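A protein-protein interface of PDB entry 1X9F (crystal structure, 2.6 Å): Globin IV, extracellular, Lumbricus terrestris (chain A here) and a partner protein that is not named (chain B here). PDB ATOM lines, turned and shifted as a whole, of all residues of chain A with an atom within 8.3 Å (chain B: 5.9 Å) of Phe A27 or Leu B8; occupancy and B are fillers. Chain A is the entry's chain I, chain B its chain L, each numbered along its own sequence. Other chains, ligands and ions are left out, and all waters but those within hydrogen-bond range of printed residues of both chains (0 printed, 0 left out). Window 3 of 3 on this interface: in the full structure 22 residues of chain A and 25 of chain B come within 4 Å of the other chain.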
ATOM      1  N   VAL A  22     -13.551  -8.334 -13.737  1.00  0.00           N
ATOM      2  CA  VAL A  22     -14.800  -7.596 -13.542  1.00  0.00           C
ATOM      3  C   VAL A  22     -15.306  -7.828 -12.116  1.00  0.00           C
ATOM      4  O   VAL A  22     -15.730  -6.890 -11.437  1.00  0.00           O
ATOM      5  CB  VAL A  22     -15.905  -7.960 -14.577  1.00  0.00           C
ATOM      6  CG1 VAL A  22     -15.345  -7.995 -15.989  1.00  0.00           C
ATOM      7  CG2 VAL A  22     -16.562  -9.278 -14.238  1.00  0.00           C
ATOM      8  N   TRP A  23     -15.233  -9.087 -11.676  1.00  0.00           N
ATOM      9  CA  TRP A  23     -15.746  -9.507 -10.374  1.00  0.00           C
ATOM     10  C   TRP A  23     -14.663  -9.471  -9.307  1.00  0.00           C
ATOM     11  O   TRP A  23     -14.182 -10.513  -8.843  1.00  0.00           O
ATOM     12  CB  TRP A  23     -16.362 -10.904 -10.450  1.00  0.00           C
ATOM     13  CG  TRP A  23     -17.280 -11.223  -9.302  1.00  0.00           C
ATOM     14  CD1 TRP A  23     -16.935 -11.750  -8.086  1.00  0.00           C
ATOM     15  CD2 TRP A  23     -18.697 -11.031  -9.264  1.00  0.00           C
ATOM     16  NE1 TRP A  23     -18.053 -11.905  -7.301  1.00  0.00           N
ATOM     17  CE2 TRP A  23     -19.149 -11.472  -7.998  1.00  0.00           C
ATOM     18  CE3 TRP A  23     -19.638 -10.533 -10.175  1.00  0.00           C
ATOM     19  CZ2 TRP A  23     -20.493 -11.431  -7.626  1.00  0.00           C
ATOM     20  CZ3 TRP A  23     -20.968 -10.490  -9.802  1.00  0.00           C
ATOM     21  CH2 TRP A  23     -21.385 -10.937  -8.537  1.00  0.00           C
ATOM     22  N   SER A  24     -14.269  -8.265  -8.920  1.00  0.00           N
ATOM     23  CA  SER A  24     -13.244  -8.160  -7.909  1.00  0.00           C
ATOM     24  C   SER A  24     -13.903  -8.096  -6.544  1.00  0.00           C
ATOM     25  O   SER A  24     -14.638  -9.015  -6.159  1.00  0.00           O
ATOM     26  CB  SER A  24     -12.334  -6.949  -8.173  1.00  0.00           C
ATOM     27  OG  SER A  24     -11.273  -6.923  -7.219  1.00  0.00           O
ATOM     28  N   SER A  25     -13.652  -6.998  -5.838  1.00  0.00           N
ATOM     29  CA  SER A  25     -14.060  -6.806  -4.455  1.00  0.00           C
ATOM     30  C   SER A  25     -15.285  -7.589  -4.008  1.00  0.00           C
ATOM     31  O   SER A  25     -16.219  -7.836  -4.788  1.00  0.00           O
ATOM     32  CB  SER A  25     -14.268  -5.313  -4.167  1.00  0.00           C
ATOM     33  OG  SER A  25     -15.438  -4.812  -4.789  1.00  0.00           O
ATOM     34  N   SER A  26     -15.261  -7.954  -2.723  1.00  0.00           N
ATOM     35  CA  SER A  26     -16.410  -8.522  -2.021  1.00  0.00           C
ATOM     36  C   SER A  26     -17.250  -7.395  -1.397  1.00  0.00           C
ATOM     37  O   SER A  26     -17.811  -7.530  -0.303  1.00  0.00           O
ATOM     38  CB  SER A  26     -15.946  -9.541  -0.970  1.00  0.00           C
ATOM     39  OG  SER A  26     -14.827  -9.068  -0.236  1.00  0.00           O
ATOM     40  N   PHE A  27     -17.283  -6.272  -2.108  1.00  0.00           N
ATOM     41  CA  PHE A  27     -18.175  -5.157  -1.852  1.00  0.00           C
ATOM     42  C   PHE A  27     -19.042  -5.081  -3.090  1.00  0.00           C
ATOM     43  O   PHE A  27     -18.656  -5.588  -4.146  1.00  0.00           O
ATOM     44  CB  PHE A  27     -17.368  -3.869  -1.691  1.00  0.00           C
ATOM     45  CG  PHE A  27     -16.580  -3.810  -0.418  1.00  0.00           C
ATOM     46  CD1 PHE A  27     -15.331  -4.423  -0.320  1.00  0.00           C
ATOM     47  CD2 PHE A  27     -17.092  -3.151   0.696  1.00  0.00           C
ATOM     48  CE1 PHE A  27     -14.601  -4.376   0.870  1.00  0.00           C
ATOM     49  CE2 PHE A  27     -16.372  -3.095   1.892  1.00  0.00           C
ATOM     50  CZ  PHE A  27     -15.124  -3.709   1.979  1.00  0.00           C
ATOM     51  N   THR A  28     -20.207  -4.455  -2.984  1.00  0.00           N
ATOM     52  CA  THR A  28     -21.130  -4.467  -4.112  1.00  0.00           C
ATOM     53  C   THR A  28     -20.953  -3.354  -5.126  1.00  0.00           C
ATOM     54  O   THR A  28     -21.423  -3.476  -6.252  1.00  0.00           O
ATOM     55  CB  THR A  28     -22.597  -4.533  -3.655  1.00  0.00           C
ATOM     56  OG1 THR A  28     -22.627  -4.477  -2.147  1.00  0.00           O
ATOM     57  CG2 THR A  28     -23.118  -5.932  -3.881  1.00  0.00           C
ATOM     58  N   ASP A  29     -20.280  -2.279  -4.735  1.00  0.00           N
ATOM     59  CA  ASP A  29     -20.194  -1.082  -5.564  1.00  0.00           C
ATOM     60  C   ASP A  29     -19.901  -1.338  -7.024  1.00  0.00           C
ATOM     61  O   ASP A  29     -20.593  -0.822  -7.904  1.00  0.00           O
ATOM     62  CB  ASP A  29     -19.128  -0.147  -5.026  1.00  0.00           C
ATOM     63  CG  ASP A  29     -19.451   0.342  -3.658  1.00  0.00           C
ATOM     64  OD1 ASP A  29     -19.894   1.506  -3.545  1.00  0.00           O
ATOM     65  OD2 ASP A  29     -19.319  -0.368  -2.636  1.00  0.00           O
ATOM     66  N   ARG A  30     -18.859  -2.114  -7.280  1.00  0.00           N
ATOM     67  CA  ARG A  30     -18.447  -2.386  -8.638  1.00  0.00           C
ATOM     68  C   ARG A  30     -19.480  -3.253  -9.368  1.00  0.00           C
ATOM     69  O   ARG A  30     -19.873  -2.935 -10.494  1.00  0.00           O
ATOM     70  CB  ARG A  30     -17.078  -3.045  -8.615  1.00  0.00           C
ATOM     71  CG  ARG A  30     -16.411  -3.137  -9.951  1.00  0.00           C
ATOM     72  CD  ARG A  30     -14.965  -3.535  -9.809  1.00  0.00           C
ATOM     73  NE  ARG A  30     -14.395  -3.879 -11.105  1.00  0.00           N
ATOM     74  CZ  ARG A  30     -13.801  -3.013 -11.914  1.00  0.00           C
ATOM     75  NH1 ARG A  30     -13.682  -1.733 -11.568  1.00  0.00           N
ATOM     76  NH2 ARG A  30     -13.315  -3.425 -13.078  1.00  0.00           N
ATOM     77  N   ARG A  31     -19.924  -4.333  -8.724  1.00  0.00           N
ATOM     78  CA  ARG A  31     -20.931  -5.206  -9.327  1.00  0.00           C
ATOM     79  C   ARG A  31     -22.320  -4.545  -9.314  1.00  0.00           C
ATOM     80  O   ARG A  31     -23.120  -4.825 -10.330  1.00  0.00           O
ATOM     81  CB  ARG A  31     -20.933  -6.599  -8.711  1.00  0.00           C
ATOM     82  CG  ARG A  31     -21.720  -6.749  -7.449  1.00  0.00           C
ATOM     83  CD  ARG A  31     -21.542  -8.120  -6.829  1.00  0.00           C
ATOM     84  NE  ARG A  31     -20.385  -8.111  -5.936  1.00  0.00           N
ATOM     85  CZ  ARG A  31     -20.142  -9.031  -5.014  1.00  0.00           C
ATOM     86  NH1 ARG A  31     -20.968 -10.068  -4.861  1.00  0.00           N
ATOM     87  NH2 ARG A  31     -19.065  -8.921  -4.243  1.00  0.00           N
ATOM     88  N   VAL A  32     -22.630  -3.628  -8.340  1.00  0.00           N
ATOM     89  CA  VAL A  32     -23.824  -2.745  -8.678  1.00  0.00           C
ATOM     90  C   VAL A  32     -23.654  -1.903  -9.980  1.00  0.00           C
ATOM     91  O   VAL A  32     -24.540  -1.947 -10.846  1.00  0.00           O
ATOM     92  CB  VAL A  32     -24.327  -1.847  -7.497  1.00  0.00           C
ATOM     93  CG1 VAL A  32     -25.381  -0.837  -7.981  1.00  0.00           C
ATOM     94  CG2 VAL A  32     -24.906  -2.693  -6.384  1.00  0.00           C
ATOM     95  N   VAL A  71     -27.531  -6.779  -7.751  1.00  0.00           N
ATOM     96  CA  VAL A  71     -26.543  -7.693  -7.201  1.00  0.00           C
ATOM     97  C   VAL A  71     -26.988  -9.134  -7.414  1.00  0.00           C
ATOM     98  O   VAL A  71     -26.157 -10.001  -7.686  1.00  0.00           O
ATOM     99  CB  VAL A  71     -26.260  -7.409  -5.700  1.00  0.00           C
ATOM    100  CG1 VAL A  71     -25.369  -8.490  -5.081  1.00  0.00           C
ATOM    101  CG2 VAL A  71     -25.627  -6.040  -5.542  1.00  0.00           C
ATOM    102  N   ASN A  75     -24.640 -11.677  -9.115  1.00  0.00           N
ATOM    103  CA  ASN A  75     -24.280 -12.970  -8.520  1.00  0.00           C
ATOM    104  C   ASN A  75     -24.813 -14.174  -9.284  1.00  0.00           C
ATOM    105  O   ASN A  75     -24.213 -15.250  -9.235  1.00  0.00           O
ATOM    106  CB  ASN A  75     -24.663 -13.054  -7.041  1.00  0.00           C
ATOM    107  CG  ASN A  75     -23.582 -12.500  -6.134  1.00  0.00           C
ATOM    108  OD1 ASN A  75     -23.355 -11.290  -6.086  1.00  0.00           O
ATOM    109  ND2 ASN A  75     -22.908 -13.384  -5.401  1.00  0.00           N
ATOM    110  N   CYS B   2     -21.948  -6.862  14.050  1.00  0.00           N
ATOM    111  CA  CYS B   2     -20.809  -6.841  13.138  1.00  0.00           C
ATOM    112  C   CYS B   2     -20.364  -5.412  12.877  1.00  0.00           C
ATOM    113  O   CYS B   2     -20.969  -4.703  12.061  1.00  0.00           O
ATOM    114  CB  CYS B   2     -21.137  -7.559  11.811  1.00  0.00           C
ATOM    115  SG  CYS B   2     -19.638  -8.346  11.101  1.00  0.00           S
ATOM    116  N   LEU B   3     -19.315  -4.991  13.573  1.00  0.00           N
ATOM    117  CA  LEU B   3     -18.686  -3.711  13.273  1.00  0.00           C
ATOM    118  C   LEU B   3     -17.967  -3.744  11.918  1.00  0.00           C
ATOM    119  O   LEU B   3     -18.066  -4.720  11.168  1.00  0.00           O
ATOM    120  CB  LEU B   3     -17.753  -3.249  14.408  1.00  0.00           C
ATOM    121  CG  LEU B   3     -16.706  -4.148  15.086  1.00  0.00           C
ATOM    122  CD1 LEU B   3     -15.592  -3.279  15.700  1.00  0.00           C
ATOM    123  CD2 LEU B   3     -17.339  -5.045  16.155  1.00  0.00           C
ATOM    124  N   VAL B   4     -17.252  -2.665  11.617  1.00  0.00           N
ATOM    125  CA  VAL B   4     -16.612  -2.471  10.322  1.00  0.00           C
ATOM    126  C   VAL B   4     -15.435  -3.415  10.123  1.00  0.00           C
ATOM    127  O   VAL B   4     -15.258  -3.972   9.037  1.00  0.00           O
ATOM    128  CB  VAL B   4     -16.101  -1.019  10.168  1.00  0.00           C
ATOM    129  CG1 VAL B   4     -15.840  -0.690   8.695  1.00  0.00           C
ATOM    130  CG2 VAL B   4     -17.101  -0.019  10.760  1.00  0.00           C
ATOM    131  N   THR B   5     -14.628  -3.576  11.168  1.00  0.00           N
ATOM    132  CA  THR B   5     -13.467  -4.456  11.107  1.00  0.00           C
ATOM    133  C   THR B   5     -13.896  -5.910  10.922  1.00  0.00           C
ATOM    134  O   THR B   5     -13.302  -6.626  10.109  1.00  0.00           O
ATOM    135  CB  THR B   5     -12.575  -4.303  12.355  1.00  0.00           C
ATOM    136  OG1 THR B   5     -13.373  -4.438  13.540  1.00  0.00           O
ATOM    137  CG2 THR B   5     -12.026  -2.887  12.457  1.00  0.00           C
ATOM    138  N   GLU B   6     -14.930  -6.334  11.647  1.00  0.00           N
ATOM    139  CA  GLU B   6     -15.406  -7.719  11.570  1.00  0.00           C
ATOM    140  C   GLU B   6     -16.018  -8.092  10.219  1.00  0.00           C
ATOM    141  O   GLU B   6     -15.741  -9.171   9.689  1.00  0.00           O
ATOM    142  CB  GLU B   6     -16.436  -7.998  12.663  1.00  0.00           C
ATOM    143  CG  GLU B   6     -15.923  -7.887  14.094  1.00  0.00           C
ATOM    144  CD  GLU B   6     -16.981  -8.340  15.085  1.00  0.00           C
ATOM    145  OE1 GLU B   6     -16.614  -8.949  16.112  1.00  0.00           O
ATOM    146  OE2 GLU B   6     -18.182  -8.099  14.834  1.00  0.00           O
ATOM    147  N   SER B   7     -16.863  -7.210   9.681  1.00  0.00           N
ATOM    148  CA  SER B   7     -17.474  -7.429   8.373  1.00  0.00           C
ATOM    149  C   SER B   7     -16.385  -7.526   7.320  1.00  0.00           C
ATOM    150  O   SER B   7     -16.475  -8.329   6.390  1.00  0.00           O
ATOM    151  CB  SER B   7     -18.454  -6.305   8.028  1.00  0.00           C
ATOM    152  OG  SER B   7     -17.782  -5.071   7.846  1.00  0.00           O
ATOM    153  N   LEU B   8     -15.345  -6.716   7.497  1.00  0.00           N
ATOM    154  CA  LEU B   8     -14.213  -6.698   6.583  1.00  0.00           C
ATOM    155  C   LEU B   8     -13.406  -7.991   6.670  1.00  0.00           C
ATOM    156  O   LEU B   8     -13.020  -8.554   5.641  1.00  0.00           O
ATOM    157  CB  LEU B   8     -13.334  -5.475   6.857  1.00  0.00           C
ATOM    158  CG  LEU B   8     -12.264  -5.031   5.853  1.00  0.00           C
ATOM    159  CD1 LEU B   8     -10.891  -5.590   6.213  1.00  0.00           C
ATOM    160  CD2 LEU B   8     -12.621  -5.372   4.397  1.00  0.00           C
ATOM    161  N   LYS B   9     -13.156  -8.449   7.898  1.00  0.00           N
ATOM    162  CA  LYS B   9     -12.502  -9.730   8.130  1.00  0.00           C
ATOM    163  C   LYS B   9     -13.282 -10.849   7.462  1.00  0.00           C
ATOM    164  O   LYS B   9     -12.690 -11.706   6.801  1.00  0.00           O
ATOM    165  CB  LYS B   9     -12.382 -10.011   9.628  1.00  0.00           C
ATOM    166  CG  LYS B   9     -11.537 -11.226   9.977  1.00  0.00           C
ATOM    167  CD  LYS B   9     -10.092 -11.025   9.557  1.00  0.00           C
ATOM    168  CE  LYS B   9      -9.128 -11.563  10.612  1.00  0.00           C
ATOM    169  NZ  LYS B   9      -9.189 -10.798  11.892  1.00  0.00           N
ATOM    170  N   VAL B  10     -14.601 -10.840   7.637  1.00  0.00           N
ATOM    171  CA  VAL B  10     -15.443 -11.893   7.072  1.00  0.00           C
ATOM    172  C   VAL B  10     -15.391 -11.853   5.542  1.00  0.00           C
ATOM    173  O   VAL B  10     -15.243 -12.895   4.901  1.00  0.00           O
ATOM    174  CB  VAL B  10     -16.908 -11.804   7.575  1.00  0.00           C
ATOM    175  CG1 VAL B  10     -17.810 -12.748   6.773  1.00  0.00           C
ATOM    176  CG2 VAL B  10     -16.991 -12.170   9.046  1.00  0.00           C
ATOM    177  N   LYS B  11     -15.507 -10.654   4.970  1.00  0.00           N
ATOM    178  CA  LYS B  11     -15.372 -10.460   3.525  1.00  0.00           C
ATOM    179  C   LYS B  11     -14.056 -11.065   3.027  1.00  0.00           C
ATOM    180  O   LYS B  11     -14.062 -11.921   2.140  1.00  0.00           O
ATOM    181  CB  LYS B  11     -15.459  -8.973   3.144  1.00  0.00           C
ATOM    182  CG  LYS B  11     -16.855  -8.347   3.238  1.00  0.00           C
ATOM    183  CD  LYS B  11     -16.796  -6.839   2.991  1.00  0.00           C
ATOM    184  CE  LYS B  11     -18.135  -6.148   3.245  1.00  0.00           C
ATOM    185  NZ  LYS B  11     -19.196  -6.568   2.284  1.00  0.00           N
ATOM    186  N   LEU B  12     -12.940 -10.630   3.612  1.00  0.00           N
ATOM    187  CA  LEU B  12     -11.622 -11.140   3.236  1.00  0.00           C
ATOM    188  C   LEU B  12     -11.510 -12.652   3.397  1.00  0.00           C
ATOM    189  O   LEU B  12     -10.989 -13.333   2.513  1.00  0.00           O
ATOM    190  CB  LEU B  12     -10.517 -10.454   4.046  1.00  0.00           C
ATOM    191  CG  LEU B  12      -9.782  -9.209   3.535  1.00  0.00           C
ATOM    192  CD1 LEU B  12     -10.609  -8.307   2.619  1.00  0.00           C
ATOM    193  CD2 LEU B  12      -9.247  -8.421   4.751  1.00  0.00           C
ATOM    194  N   GLN B  13     -11.992 -13.178   4.521  1.00  0.00           N
ATOM    195  CA  GLN B  13     -11.853 -14.612   4.768  1.00  0.00           C
ATOM    196  C   GLN B  13     -12.766 -15.427   3.865  1.00  0.00           C
ATOM    197  O   GLN B  13     -12.402 -16.535   3.469  1.00  0.00           O
ATOM    198  CB  GLN B  13     -12.091 -14.958   6.244  1.00  0.00           C
ATOM    199  CG  GLN B  13     -11.025 -14.394   7.176  1.00  0.00           C
ATOM    200  CD  GLN B  13     -10.884 -15.164   8.476  1.00  0.00           C
ATOM    201  OE1 GLN B  13     -11.870 -15.465   9.153  1.00  0.00           O
ATOM    202  NE2 GLN B  13      -9.641 -15.463   8.848  1.00  0.00           N
ATOM    203  N   SER B  75     -21.206  -9.919   0.992  1.00  0.00           N
ATOM    204  CA  SER B  75     -20.805  -8.695   0.299  1.00  0.00           C
ATOM    205  C   SER B  75     -21.692  -7.484   0.632  1.00  0.00           C
ATOM    206  O   SER B  75     -21.373  -6.350   0.268  1.00  0.00           O
ATOM    207  CB  SER B  75     -20.748  -8.925  -1.205  1.00  0.00           C
ATOM    208  OG  SER B  75     -22.040  -9.216  -1.709  1.00  0.00           O
ATOM    209  N   ASP B  78     -21.921  -4.393   4.809  1.00  0.00           N
ATOM    210  CA  ASP B  78     -21.637  -2.980   5.044  1.00  0.00           C
ATOM    211  C   ASP B  78     -22.671  -2.030   4.430  1.00  0.00           C
ATOM    212  O   ASP B  78     -22.525  -0.809   4.533  1.00  0.00           O
ATOM    213  CB  ASP B  78     -20.252  -2.638   4.494  1.00  0.00           C
ATOM    214  CG  ASP B  78     -20.148  -2.898   3.003  1.00  0.00           C
ATOM    215  OD1 ASP B  78     -19.600  -2.034   2.282  1.00  0.00           O
ATOM    216  OD2 ASP B  78     -20.597  -3.936   2.458  1.00  0.00           O
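The side-chain amino group of Lys B11 lies within hydrogen-bond range of the backbone carbonyl oxygen of Ser A26 (3.1 Å). The side-chain hydroxyl of Thr A28 lies within hydrogen-bond range of the backbone carbonyl oxygen of Ser B75 (3.3 Å). The side-chain hydroxyl of Ser B75 is in hydrogen-bond range of the guanidinium group of Arg A31 (3.4 Å).
OG of Ser A25 is in hydrogen-bond range of O of Phe A27 (3.4 Å). NH2 of Arg A31 is in hydrogen-bond range of O of Ser A25. The guanidinium group (NH2) of Arg A31 sits at hydrogen-bond distance from the backbone carbonyl oxygen (O) of Phe A27 (3.4 Å). The guanidinium group (NH1) of Arg A31 is in hydrogen-bond range of the side-chain amide oxygen (OD1) of Asn A75 (2.9 Å). NZ of Lys B11 is in hydrogen-bond range of O of Ser B75 (3.0 Å). The side-chain amino group of Lys B11 lies within salt-bridge range of the side-chain carboxylate of Asp B78 (3.0 Å).
Among the printed residues, pairs that only touch across the chains: Ser A26 with Ser B75 (3.3 Å), Phe A27 with Leu B8 (3.9 Å), Phe A27 with Lys B11 (3.7 Å) and Phe A27 with Asp B78 (3.2 Å).
Of chain A, only Phe A27 comes within 4 Å of Leu B8. No residue of chain A comes within 4 Å of Ser B7. Of the printed residues of chain B, Arg A31 touches Ser B75. Of the printed residues of chain A, Asp B78 touches Phe A27 (3.2 Å). The nearest printed residue of chain B that does not touch Phe A27 is Ser B75 (4.02 Å). The nearest residue of chain A that does not touch Leu B8 is Ser A26 (6.2 Å). The nearest printed residue of chain B that does not touch Arg A31 is Lys B11 (6.9 Å).
Hydrophobic or aromatic side chains of chain B that line the printed part of chain A: Leu B8. Among the printed residues, no Asp or Glu carboxylate lies within 4 Å of a Lys or Arg side-chain nitrogen of the other chain.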
